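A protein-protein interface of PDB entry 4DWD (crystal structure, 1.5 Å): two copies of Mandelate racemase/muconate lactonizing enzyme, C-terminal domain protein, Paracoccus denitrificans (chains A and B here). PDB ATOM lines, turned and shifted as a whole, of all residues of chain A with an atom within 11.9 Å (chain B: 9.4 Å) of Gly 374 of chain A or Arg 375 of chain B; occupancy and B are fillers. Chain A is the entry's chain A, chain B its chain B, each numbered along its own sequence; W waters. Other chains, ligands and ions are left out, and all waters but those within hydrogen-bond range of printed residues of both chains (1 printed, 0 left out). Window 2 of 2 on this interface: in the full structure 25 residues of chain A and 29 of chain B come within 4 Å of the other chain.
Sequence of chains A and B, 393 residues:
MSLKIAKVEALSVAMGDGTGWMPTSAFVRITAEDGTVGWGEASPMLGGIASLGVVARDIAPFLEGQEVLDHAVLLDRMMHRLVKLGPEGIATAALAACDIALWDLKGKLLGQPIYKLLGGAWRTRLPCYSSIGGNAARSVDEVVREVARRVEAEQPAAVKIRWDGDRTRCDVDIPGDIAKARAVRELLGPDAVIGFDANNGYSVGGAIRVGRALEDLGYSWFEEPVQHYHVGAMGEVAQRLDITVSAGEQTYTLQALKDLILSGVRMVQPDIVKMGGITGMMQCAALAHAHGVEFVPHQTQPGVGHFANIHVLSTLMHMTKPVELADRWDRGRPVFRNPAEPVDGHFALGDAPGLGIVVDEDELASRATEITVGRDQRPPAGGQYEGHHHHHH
N of Asp 376 of chain B sits at hydrogen-bond distance from O of Gly 374 of chain A (3.2 Å).
The backbone NH of Ala 50 of chain A lies close to the guanidinium group of Arg 57 of chain B (3.5 Å).
OG1 of Thr 372 of chain B sits close to O of Arg 375 of chain B.
Arg 57 of chain B touches Ile 49 of chain A (NE to CG2, 3.5 Å).
Ile 49 of chain B touches Arg 57 of chain A (CG2 to NE, 3.5 Å).
CB of Arg 375 of chain B touches O of Gly 374 of chain A, at 3.99 Å.
Of the printed residues of chain B, Ile 49 of chain A touches Arg 57 (3.5 Å).
Of the printed residues of chain B, Ala 50 of chain A touches Arg 57.
Printed residues of chain B within 4 Å of Arg 57 of chain A: Ile 49 (3.5 Å).
No residue of chain B comes within 4 Å of Val 373 of chain A.
Of the printed residues of chain B, Gly 374 of chain A touches Arg 375 and Asp 376.
No residue of chain A comes within 4 Å of Ile 371 of chain B.
No residue of chain A comes within 4 Å of Thr 372 of chain B.
No residue of chain A comes within 4 Å of Val 373 of chain B.
No residue of chain A comes within 4 Å of Gly 374 of chain B.
Printed residues of chain A within 4 Å of Arg 375 of chain B: Gly 374 (3.99 Å).
Asp 376 of chain B touches just one residue of chain A: Gly 374 (3.2 Å).
No residue of chain A comes within 4 Å of Gln 377 of chain B.
The nearest printed residue of chain B that does not touch Gly 374 of chain A is Gly 374 of chain B (5.4 Å).
Printed residues of chain A that touch a printed residue of chain B: Ile 49, Ala 50, Arg 57 and Gly 374.
Of the 17 printed residues of chain B, 4 touch a printed residue of chain A.
Among the printed residues, no Asp or Glu carboxylate lies within 4 Å of a Lys or Arg side-chain nitrogen of the other chain.
Ile 49 of chain A touches Arg 57 of chain B, and with the chains exchanged Arg 57 of chain A touches Ile 49 of chain B.
Of the 5 pairs that touch across the chains among the printed residues, 2 have their exchanged pair printed and touching as well.
Water W1 bridges NH1 of Arg 57 of chain B (3.2 Å) and NH1 of Arg 57 of chain A (3.5 Å).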
ATOM      1  N   ALA A  10      -4.863 -21.435 -25.354  1.00  0.00           N
ATOM      2  CA  ALA A  10      -4.534 -22.849 -25.513  1.00  0.00           C
ATOM      3  C   ALA A  10      -5.473 -23.440 -26.556  1.00  0.00           C
ATOM      4  O   ALA A  10      -6.694 -23.400 -26.372  1.00  0.00           O
ATOM      5  CB  ALA A  10      -4.688 -23.573 -24.181  1.00  0.00           C
ATOM      6  N   ILE A  49      -4.312 -32.515 -24.503  1.00  0.00           N
ATOM      7  CA  ILE A  49      -5.412 -31.803 -23.827  1.00  0.00           C
ATOM      8  C   ILE A  49      -5.059 -31.438 -22.380  1.00  0.00           C
ATOM      9  O   ILE A  49      -5.353 -30.328 -21.915  1.00  0.00           O
ATOM     10  CB  ILE A  49      -6.733 -32.611 -23.887  1.00  0.00           C
ATOM     11  CG1 ILE A  49      -7.107 -32.946 -25.342  1.00  0.00           C
ATOM     12  CG2 ILE A  49      -7.872 -31.878 -23.177  1.00  0.00           C
ATOM     13  CD1 ILE A  49      -7.224 -31.761 -26.287  1.00  0.00           C
ATOM     14  N   ALA A  50      -4.418 -32.358 -21.661  1.00  0.00           N
ATOM     15  CA  ALA A  50      -4.025 -32.057 -20.286  1.00  0.00           C
ATOM     16  C   ALA A  50      -3.037 -30.880 -20.227  1.00  0.00           C
ATOM     17  O   ALA A  50      -3.197 -29.986 -19.396  1.00  0.00           O
ATOM     18  CB  ALA A  50      -3.447 -33.288 -19.600  1.00  0.00           C
ATOM     19  N   LEU A  52      -2.763 -28.482 -22.440  1.00  0.00           N
ATOM     20  CA  LEU A  52      -3.532 -27.289 -22.785  1.00  0.00           C
ATOM     21  C   LEU A  52      -4.340 -26.769 -21.598  1.00  0.00           C
ATOM     22  O   LEU A  52      -4.413 -25.551 -21.381  1.00  0.00           O
ATOM     23  CB  LEU A  52      -4.436 -27.552 -23.993  1.00  0.00           C
ATOM     24  CG  LEU A  52      -3.674 -27.770 -25.310  1.00  0.00           C
ATOM     25  CD1 LEU A  52      -4.689 -28.131 -26.394  1.00  0.00           C
ATOM     26  CD2 LEU A  52      -2.866 -26.551 -25.736  1.00  0.00           C
ATOM     27  N   GLY A  53      -4.937 -27.682 -20.829  1.00  0.00           N
ATOM     28  CA  GLY A  53      -5.648 -27.297 -19.599  1.00  0.00           C
ATOM     29  C   GLY A  53      -4.739 -26.628 -18.576  1.00  0.00           C
ATOM     30  O   GLY A  53      -5.124 -25.652 -17.945  1.00  0.00           O
ATOM     31  N   VAL A  54      -3.531 -27.165 -18.408  1.00  0.00           N
ATOM     32  CA  VAL A  54      -2.526 -26.549 -17.527  1.00  0.00           C
ATOM     33  C   VAL A  54      -2.142 -25.135 -18.000  1.00  0.00           C
ATOM     34  O   VAL A  54      -2.036 -24.222 -17.190  1.00  0.00           O
ATOM     35  CB  VAL A  54      -1.309 -27.493 -17.332  1.00  0.00           C
ATOM     36  CG1 VAL A  54      -0.137 -26.770 -16.683  1.00  0.00           C
ATOM     37  CG2 VAL A  54      -1.715 -28.694 -16.475  1.00  0.00           C
ATOM     38  N   VAL A  55      -1.961 -24.950 -19.306  1.00  0.00           N
ATOM     39  CA  VAL A  55      -1.724 -23.603 -19.848  1.00  0.00           C
ATOM     40  C   VAL A  55      -2.886 -22.667 -19.468  1.00  0.00           C
ATOM     41  O   VAL A  55      -2.678 -21.594 -18.878  1.00  0.00           O
ATOM     42  CB  VAL A  55      -1.530 -23.618 -21.382  1.00  0.00           C
ATOM     43  CG1 VAL A  55      -1.434 -22.195 -21.918  1.00  0.00           C
ATOM     44  CG2 VAL A  55      -0.274 -24.393 -21.770  1.00  0.00           C
ATOM     45  N   ALA A  56      -4.110 -23.078 -19.789  1.00  0.00           N
ATOM     46  CA  ALA A  56      -5.268 -22.204 -19.613  1.00  0.00           C
ATOM     47  C   ALA A  56      -5.536 -21.852 -18.139  1.00  0.00           C
ATOM     48  O   ALA A  56      -5.770 -20.685 -17.813  1.00  0.00           O
ATOM     49  CB  ALA A  56      -6.494 -22.830 -20.257  1.00  0.00           C
ATOM     50  N   ARG A  57      -5.490 -22.857 -17.265  1.00  0.00           N
ATOM     51  CA  ARG A  57      -5.812 -22.677 -15.844  1.00  0.00           C
ATOM     52  C   ARG A  57      -4.663 -22.113 -15.018  1.00  0.00           C
ATOM     53  O   ARG A  57      -4.884 -21.281 -14.139  1.00  0.00           O
ATOM     54  CB  ARG A  57      -6.195 -24.016 -15.196  1.00  0.00           C
ATOM     55  CG  ARG A  57      -7.595 -24.539 -15.436  1.00  0.00           C
ATOM     56  CD  ARG A  57      -7.894 -25.685 -14.462  1.00  0.00           C
ATOM     57  NE  ARG A  57      -6.867 -26.733 -14.488  1.00  0.00           N
ATOM     58  CZ  ARG A  57      -6.738 -27.656 -15.441  1.00  0.00           C
ATOM     59  NH1 ARG A  57      -7.577 -27.696 -16.475  1.00  0.00           N
ATOM     60  NH2 ARG A  57      -5.755 -28.540 -15.361  1.00  0.00           N
ATOM     61  N   ASP A  58      -3.446 -22.592 -15.273  1.00  0.00           N
ATOM     62  CA  ASP A  58      -2.332 -22.396 -14.336  1.00  0.00           C
ATOM     63  C   ASP A  58      -1.285 -21.409 -14.814  1.00  0.00           C
ATOM     64  O   ASP A  58      -0.650 -20.763 -13.991  1.00  0.00           O
ATOM     65  CB  ASP A  58      -1.630 -23.723 -13.993  1.00  0.00           C
ATOM     66  CG  ASP A  58      -2.584 -24.800 -13.493  1.00  0.00           C
ATOM     67  OD1 ASP A  58      -3.542 -24.488 -12.746  1.00  0.00           O
ATOM     68  OD2 ASP A  58      -2.361 -25.982 -13.839  1.00  0.00           O
ATOM     69  N   ILE A  59      -1.056 -21.333 -16.128  1.00  0.00           N
ATOM     70  CA  ILE A  59       0.023 -20.509 -16.660  1.00  0.00           C
ATOM     71  C   ILE A  59      -0.489 -19.186 -17.204  1.00  0.00           C
ATOM     72  O   ILE A  59       0.038 -18.131 -16.852  1.00  0.00           O
ATOM     73  CB  ILE A  59       0.841 -21.256 -17.743  1.00  0.00           C
ATOM     74  CG1 ILE A  59       1.462 -22.529 -17.155  1.00  0.00           C
ATOM     75  CG2 ILE A  59       1.931 -20.351 -18.322  1.00  0.00           C
ATOM     76  CD1 ILE A  59       2.065 -23.451 -18.197  1.00  0.00           C
ATOM     77  N   ALA A  60      -1.522 -19.245 -18.048  1.00  0.00           N
ATOM     78  CA  ALA A  60      -2.053 -18.050 -18.717  1.00  0.00           C
ATOM     79  C   ALA A  60      -2.360 -16.875 -17.770  1.00  0.00           C
ATOM     80  O   ALA A  60      -1.916 -15.755 -18.036  1.00  0.00           O
ATOM     81  CB  ALA A  60      -3.271 -18.406 -19.562  1.00  0.00           C
ATOM     82  N   PRO A  61      -3.104 -17.117 -16.666  1.00  0.00           N
ATOM     83  CA  PRO A  61      -3.420 -15.978 -15.790  1.00  0.00           C
ATOM     84  C   PRO A  61      -2.177 -15.270 -15.233  1.00  0.00           C
ATOM     85  O   PRO A  61      -2.205 -14.058 -15.013  1.00  0.00           O
ATOM     86  CB  PRO A  61      -4.240 -16.611 -14.655  1.00  0.00           C
ATOM     87  CG  PRO A  61      -4.790 -17.874 -15.228  1.00  0.00           C
ATOM     88  CD  PRO A  61      -3.768 -18.357 -16.214  1.00  0.00           C
ATOM     89  N   THR A 369     -10.186 -25.635 -31.458  1.00  0.00           N
ATOM     90  CA  THR A 369     -11.042 -25.569 -30.292  1.00  0.00           C
ATOM     91  C   THR A 369     -10.228 -24.961 -29.167  1.00  0.00           C
ATOM     92  O   THR A 369      -9.146 -25.463 -28.826  1.00  0.00           O
ATOM     93  CB  THR A 369     -11.557 -26.965 -29.894  1.00  0.00           C
ATOM     94  OG1 THR A 369     -12.377 -27.475 -30.950  1.00  0.00           O
ATOM     95  CG2 THR A 369     -12.390 -26.902 -28.603  1.00  0.00           C
ATOM     96  N   GLU A 370     -10.723 -23.856 -28.620  1.00  0.00           N
ATOM     97  CA  GLU A 370     -10.063 -23.238 -27.489  1.00  0.00           C
ATOM     98  C   GLU A 370     -10.327 -24.040 -26.228  1.00  0.00           C
ATOM     99  O   GLU A 370     -11.468 -24.429 -25.949  1.00  0.00           O
ATOM    100  CB  GLU A 370     -10.494 -21.778 -27.304  1.00  0.00           C
ATOM    101  CG  GLU A 370      -9.746 -21.130 -26.149  1.00  0.00           C
ATOM    102  CD  GLU A 370      -9.119 -19.799 -26.481  1.00  0.00           C
ATOM    103  OE1 GLU A 370      -8.962 -19.474 -27.685  1.00  0.00           O
ATOM    104  OE2 GLU A 370      -8.761 -19.090 -25.511  1.00  0.00           O
ATOM    105  N   ILE A 371      -9.260 -24.289 -25.474  1.00  0.00           N
ATOM    106  CA  ILE A 371      -9.359 -24.948 -24.185  1.00  0.00           C
ATOM    107  C   ILE A 371      -9.371 -23.847 -23.140  1.00  0.00           C
ATOM    108  O   ILE A 371      -8.415 -23.090 -23.011  1.00  0.00           O
ATOM    109  CB  ILE A 371      -8.185 -25.934 -23.967  1.00  0.00           C
ATOM    110  CG1 ILE A 371      -8.147 -26.994 -25.080  1.00  0.00           C
ATOM    111  CG2 ILE A 371      -8.258 -26.569 -22.585  1.00  0.00           C
ATOM    112  CD1 ILE A 371      -9.437 -27.770 -25.294  1.00  0.00           C
ATOM    113  N   THR A 372     -10.471 -23.752 -22.410  1.00  0.00           N
ATOM    114  CA  THR A 372     -10.661 -22.652 -21.468  1.00  0.00           C
ATOM    115  C   THR A 372     -10.827 -23.183 -20.064  1.00  0.00           C
ATOM    116  O   THR A 372     -11.119 -24.363 -19.865  1.00  0.00           O
ATOM    117  CB  THR A 372     -11.918 -21.834 -21.808  1.00  0.00           C
ATOM    118  OG1 THR A 372     -13.049 -22.703 -21.819  1.00  0.00           O
ATOM    119  CG2 THR A 372     -11.789 -21.183 -23.170  1.00  0.00           C
ATOM    120  N   VAL A 373     -10.664 -22.300 -19.089  1.00  0.00           N
ATOM    121  CA  VAL A 373     -10.875 -22.679 -17.701  1.00  0.00           C
ATOM    122  C   VAL A 373     -12.311 -23.177 -17.553  1.00  0.00           C
ATOM    123  O   VAL A 373     -13.263 -22.487 -17.941  1.00  0.00           O
ATOM    124  CB  VAL A 373     -10.580 -21.521 -16.738  1.00  0.00           C
ATOM    125  CG1 VAL A 373     -10.778 -21.972 -15.302  1.00  0.00           C
ATOM    126  CG2 VAL A 373      -9.159 -21.027 -16.933  1.00  0.00           C
ATOM    127  N   GLY A 374     -12.420 -24.377 -16.979  1.00  0.00           N
ATOM    128  CA  GLY A 374     -13.639 -25.211 -16.951  1.00  0.00           C
ATOM    129  C   GLY A 374     -14.691 -25.023 -18.034  1.00  0.00           C
ATOM    130  O   GLY A 374     -15.812 -25.519 -17.889  1.00  0.00           O
ATOM    131  N   ALA B  10     -15.133 -38.229 -11.738  1.00  0.00           N
ATOM    132  CA  ALA B  10     -14.042 -37.385 -11.249  1.00  0.00           C
ATOM    133  C   ALA B  10     -14.653 -36.123 -10.637  1.00  0.00           C
ATOM    134  O   ALA B  10     -15.350 -35.377 -11.327  1.00  0.00           O
ATOM    135  CB  ALA B  10     -13.101 -37.024 -12.397  1.00  0.00           C
ATOM    136  N   SER B  12     -14.304 -32.594  -8.197  1.00  0.00           N
ATOM    137  CA  SER B  12     -13.588 -31.525  -7.519  1.00  0.00           C
ATOM    138  C   SER B  12     -14.512 -31.030  -6.409  1.00  0.00           C
ATOM    139  O   SER B  12     -15.631 -30.575  -6.687  1.00  0.00           O
ATOM    140  CB  SER B  12     -13.256 -30.396  -8.503  1.00  0.00           C
ATOM    141  OG  SER B  12     -12.753 -29.248  -7.836  1.00  0.00           O
ATOM    142  N   ILE B  49      -7.039 -30.694 -10.582  1.00  0.00           N
ATOM    143  CA  ILE B  49      -7.941 -30.600 -11.735  1.00  0.00           C
ATOM    144  C   ILE B  49      -7.387 -31.343 -12.950  1.00  0.00           C
ATOM    145  O   ILE B  49      -8.124 -32.062 -13.629  1.00  0.00           O
ATOM    146  CB  ILE B  49      -8.261 -29.126 -12.086  1.00  0.00           C
ATOM    147  CG1 ILE B  49      -8.807 -28.374 -10.854  1.00  0.00           C
ATOM    148  CG2 ILE B  49      -9.215 -29.051 -13.280  1.00  0.00           C
ATOM    149  CD1 ILE B  49     -10.060 -28.956 -10.246  1.00  0.00           C
ATOM    150  N   LEU B  52      -7.920 -35.021 -12.383  1.00  0.00           N
ATOM    151  CA  LEU B  52      -9.326 -35.335 -12.583  1.00  0.00           C
ATOM    152  C   LEU B  52      -9.703 -35.376 -14.068  1.00  0.00           C
ATOM    153  O   LEU B  52     -10.484 -36.238 -14.479  1.00  0.00           O
ATOM    154  CB  LEU B  52     -10.206 -34.341 -11.825  1.00  0.00           C
ATOM    155  CG  LEU B  52     -10.132 -34.395 -10.290  1.00  0.00           C
ATOM    156  CD1 LEU B  52     -11.005 -33.281  -9.713  1.00  0.00           C
ATOM    157  CD2 LEU B  52     -10.555 -35.754  -9.737  1.00  0.00           C
ATOM    158  N   GLY B  53      -9.132 -34.474 -14.861  1.00  0.00           N
ATOM    159  CA  GLY B  53      -9.324 -34.494 -16.310  1.00  0.00           C
ATOM    160  C   GLY B  53      -8.766 -35.756 -16.956  1.00  0.00           C
ATOM    161  O   GLY B  53      -9.379 -36.325 -17.863  1.00  0.00           O
ATOM    162  N   ALA B  56     -11.255 -38.519 -16.174  1.00  0.00           N
ATOM    163  CA  ALA B  56     -12.478 -38.416 -16.972  1.00  0.00           C
ATOM    164  C   ALA B  56     -12.254 -38.752 -18.452  1.00  0.00           C
ATOM    165  O   ALA B  56     -13.055 -39.462 -19.062  1.00  0.00           O
ATOM    166  CB  ALA B  56     -13.083 -37.027 -16.836  1.00  0.00           C
ATOM    167  N   ARG B  57     -11.168 -38.245 -19.029  1.00  0.00           N
ATOM    168  CA  ARG B  57     -10.956 -38.402 -20.471  1.00  0.00           C
ATOM    169  C   ARG B  57     -10.275 -39.714 -20.831  1.00  0.00           C
ATOM    170  O   ARG B  57     -10.595 -40.328 -21.852  1.00  0.00           O
ATOM    171  CB  ARG B  57     -10.096 -37.265 -21.024  1.00  0.00           C
ATOM    172  CG  ARG B  57     -10.734 -35.890 -21.082  1.00  0.00           C
ATOM    173  CD  ARG B  57      -9.853 -34.943 -21.896  1.00  0.00           C
ATOM    174  NE  ARG B  57      -8.486 -34.857 -21.368  1.00  0.00           N
ATOM    175  CZ  ARG B  57      -8.129 -34.103 -20.329  1.00  0.00           C
ATOM    176  NH1 ARG B  57      -9.024 -33.344 -19.706  1.00  0.00           N
ATOM    177  NH2 ARG B  57      -6.876 -34.099 -19.918  1.00  0.00           N
ATOM    178  N   THR B 369     -18.080 -30.504  -7.951  1.00  0.00           N
ATOM    179  CA  THR B 369     -18.173 -30.180  -9.361  1.00  0.00           C
ATOM    180  C   THR B 369     -17.621 -31.383 -10.106  1.00  0.00           C
ATOM    181  O   THR B 369     -16.480 -31.790  -9.874  1.00  0.00           O
ATOM    182  CB  THR B 369     -17.340 -28.926  -9.694  1.00  0.00           C
ATOM    183  OG1 THR B 369     -17.893 -27.791  -9.013  1.00  0.00           O
ATOM    184  CG2 THR B 369     -17.334 -28.644 -11.194  1.00  0.00           C
ATOM    185  N   GLU B 370     -18.425 -31.964 -10.986  1.00  0.00           N
ATOM    186  CA  GLU B 370     -17.918 -33.052 -11.800  1.00  0.00           C
ATOM    187  C   GLU B 370     -17.033 -32.529 -12.920  1.00  0.00           C
ATOM    188  O   GLU B 370     -17.371 -31.556 -13.598  1.00  0.00           O
ATOM    189  CB  GLU B 370     -19.029 -33.938 -12.365  1.00  0.00           C
ATOM    190  CG  GLU B 370     -18.449 -35.243 -12.913  1.00  0.00           C
ATOM    191  CD  GLU B 370     -19.472 -36.172 -13.534  1.00  0.00           C
ATOM    192  OE1 GLU B 370     -20.662 -35.803 -13.587  1.00  0.00           O
ATOM    193  OE2 GLU B 370     -19.082 -37.276 -13.982  1.00  0.00           O
ATOM    194  N   ILE B 371     -15.893 -33.187 -13.101  1.00  0.00           N
ATOM    195  CA  ILE B 371     -14.991 -32.891 -14.196  1.00  0.00           C
ATOM    196  C   ILE B 371     -15.307 -33.907 -15.267  1.00  0.00           C
ATOM    197  O   ILE B 371     -15.215 -35.102 -15.037  1.00  0.00           O
ATOM    198  CB  ILE B 371     -13.521 -33.020 -13.751  1.00  0.00           C
ATOM    199  CG1 ILE B 371     -13.240 -32.125 -12.532  1.00  0.00           C
ATOM    200  CG2 ILE B 371     -12.566 -32.761 -14.915  1.00  0.00           C
ATOM    201  CD1 ILE B 371     -13.550 -30.654 -12.713  1.00  0.00           C
ATOM    202  N   THR B 372     -15.738 -33.430 -16.423  1.00  0.00           N
ATOM    203  CA  THR B 372     -16.190 -34.334 -17.467  1.00  0.00           C
ATOM    204  C   THR B 372     -15.376 -34.135 -18.719  1.00  0.00           C
ATOM    205  O   THR B 372     -14.574 -33.212 -18.805  1.00  0.00           O
ATOM    206  CB  THR B 372     -17.680 -34.122 -17.817  1.00  0.00           C
ATOM    207  OG1 THR B 372     -17.868 -32.791 -18.311  1.00  0.00           O
ATOM    208  CG2 THR B 372     -18.578 -34.352 -16.604  1.00  0.00           C
ATOM    209  N   VAL B 373     -15.583 -35.012 -19.693  1.00  0.00           N
ATOM    210  CA  VAL B 373     -14.959 -34.843 -20.989  1.00  0.00           C
ATOM    211  C   VAL B 373     -15.489 -33.542 -21.580  1.00  0.00           C
ATOM    212  O   VAL B 373     -16.691 -33.396 -21.825  1.00  0.00           O
ATOM    213  CB  VAL B 373     -15.243 -36.046 -21.903  1.00  0.00           C
ATOM    214  CG1 VAL B 373     -14.740 -35.793 -23.318  1.00  0.00           C
ATOM    215  CG2 VAL B 373     -14.604 -37.291 -21.311  1.00  0.00           C
ATOM    216  N   GLY B 374     -14.583 -32.581 -21.739  1.00  0.00           N
ATOM    217  CA  GLY B 374     -14.910 -31.295 -22.331  1.00  0.00           C
ATOM    218  C   GLY B 374     -15.368 -30.162 -21.425  1.00  0.00           C
ATOM    219  O   GLY B 374     -15.671 -29.090 -21.943  1.00  0.00           O
ATOM    220  N   ARG B 375     -15.427 -30.368 -20.099  1.00  0.00           N
ATOM    221  CA  ARG B 375     -15.905 -29.306 -19.166  1.00  0.00           C
ATOM    222  C   ARG B 375     -15.928 -29.569 -17.629  1.00  0.00           C
ATOM    223  O   ARG B 375     -15.625 -30.666 -17.142  1.00  0.00           O
ATOM    224  CB  ARG B 375     -17.297 -28.795 -19.609  1.00  0.00           C
ATOM    225  CG  ARG B 375     -18.379 -29.873 -19.722  1.00  0.00           C
ATOM    226  CD  ARG B 375     -19.535 -29.442 -20.615  1.00  0.00           C
ATOM    227  NE  ARG B 375     -19.088 -29.066 -21.958  1.00  0.00           N
ATOM    228  CZ  ARG B 375     -19.814 -29.190 -23.070  1.00  0.00           C
ATOM    229  NH1 ARG B 375     -19.301 -28.810 -24.236  1.00  0.00           N
ATOM    230  NH2 ARG B 375     -21.045 -29.696 -23.029  1.00  0.00           N
ATOM    231  N   ASP B 376     -16.273 -28.517 -16.881  1.00  0.00           N
ATOM    232  CA  ASP B 376     -16.626 -28.610 -15.461  1.00  0.00           C
ATOM    233  C   ASP B 376     -18.148 -28.484 -15.357  1.00  0.00           C
ATOM    234  O   ASP B 376     -18.747 -27.634 -16.014  1.00  0.00           O
ATOM    235  CB  ASP B 376     -15.989 -27.472 -14.650  1.00  0.00           C
ATOM    236  CG  ASP B 376     -14.465 -27.568 -14.554  1.00  0.00           C
ATOM    237  OD1 ASP B 376     -13.840 -28.333 -15.318  1.00  0.00           O
ATOM    238  OD2 ASP B 376     -13.884 -26.851 -13.712  1.00  0.00           O
ATOM    239  N   GLN B 377     -18.769 -29.330 -14.539  1.00  0.00           N
ATOM    240  CA  GLN B 377     -20.219 -29.276 -14.322  1.00  0.00           C
ATOM    241  C   GLN B 377     -20.587 -28.932 -12.877  1.00  0.00           C
ATOM    242  O   GLN B 377     -20.393 -29.753 -11.971  1.00  0.00           O
ATOM    243  CB  GLN B 377     -20.877 -30.599 -14.732  1.00  0.00           C
ATOM    244  CG  GLN B 377     -21.054 -30.768 -16.233  1.00  0.00           C
ATOM    245  CD  GLN B 377     -21.807 -32.034 -16.605  1.00  0.00           C
ATOM    246  OE1 GLN B 377     -22.253 -32.793 -15.739  1.00  0.00           O
ATOM    247  NE2 GLN B 377     -21.954 -32.269 -17.907  1.00  0.00           N
ATOM    248  N   ARG B 378     -21.088 -27.707 -12.691  1.00  0.00           N
ATOM    249  CA  ARG B 378     -21.664 -27.183 -11.435  1.00  0.00           C
ATOM    250  C   ARG B 378     -21.384 -25.692 -11.259  1.00  0.00           C
ATOM    251  O   ARG B 378     -20.396 -25.168 -11.776  1.00  0.00           O
ATOM    252  CB  ARG B 378     -21.213 -27.957 -10.192  1.00  0.00           C
ATOM    253  CG  ARG B 378     -22.326 -28.754  -9.520  1.00  0.00           C
ATOM    254  CD  ARG B 378     -23.000 -27.974  -8.401  1.00  0.00           C
ATOM    255  NE  ARG B 378     -22.257 -28.045  -7.139  1.00  0.00           N
ATOM    256  CZ  ARG B 378     -21.251 -27.239  -6.798  1.00  0.00           C
ATOM    257  NH1 ARG B 378     -20.832 -26.284  -7.622  1.00  0.00           N
ATOM    258  NH2 ARG B 378     -20.647 -27.391  -5.626  1.00  0.00           N
HETATM  259  O   HOH W   1      -8.172 -30.711 -18.087  1.00  0.00           O
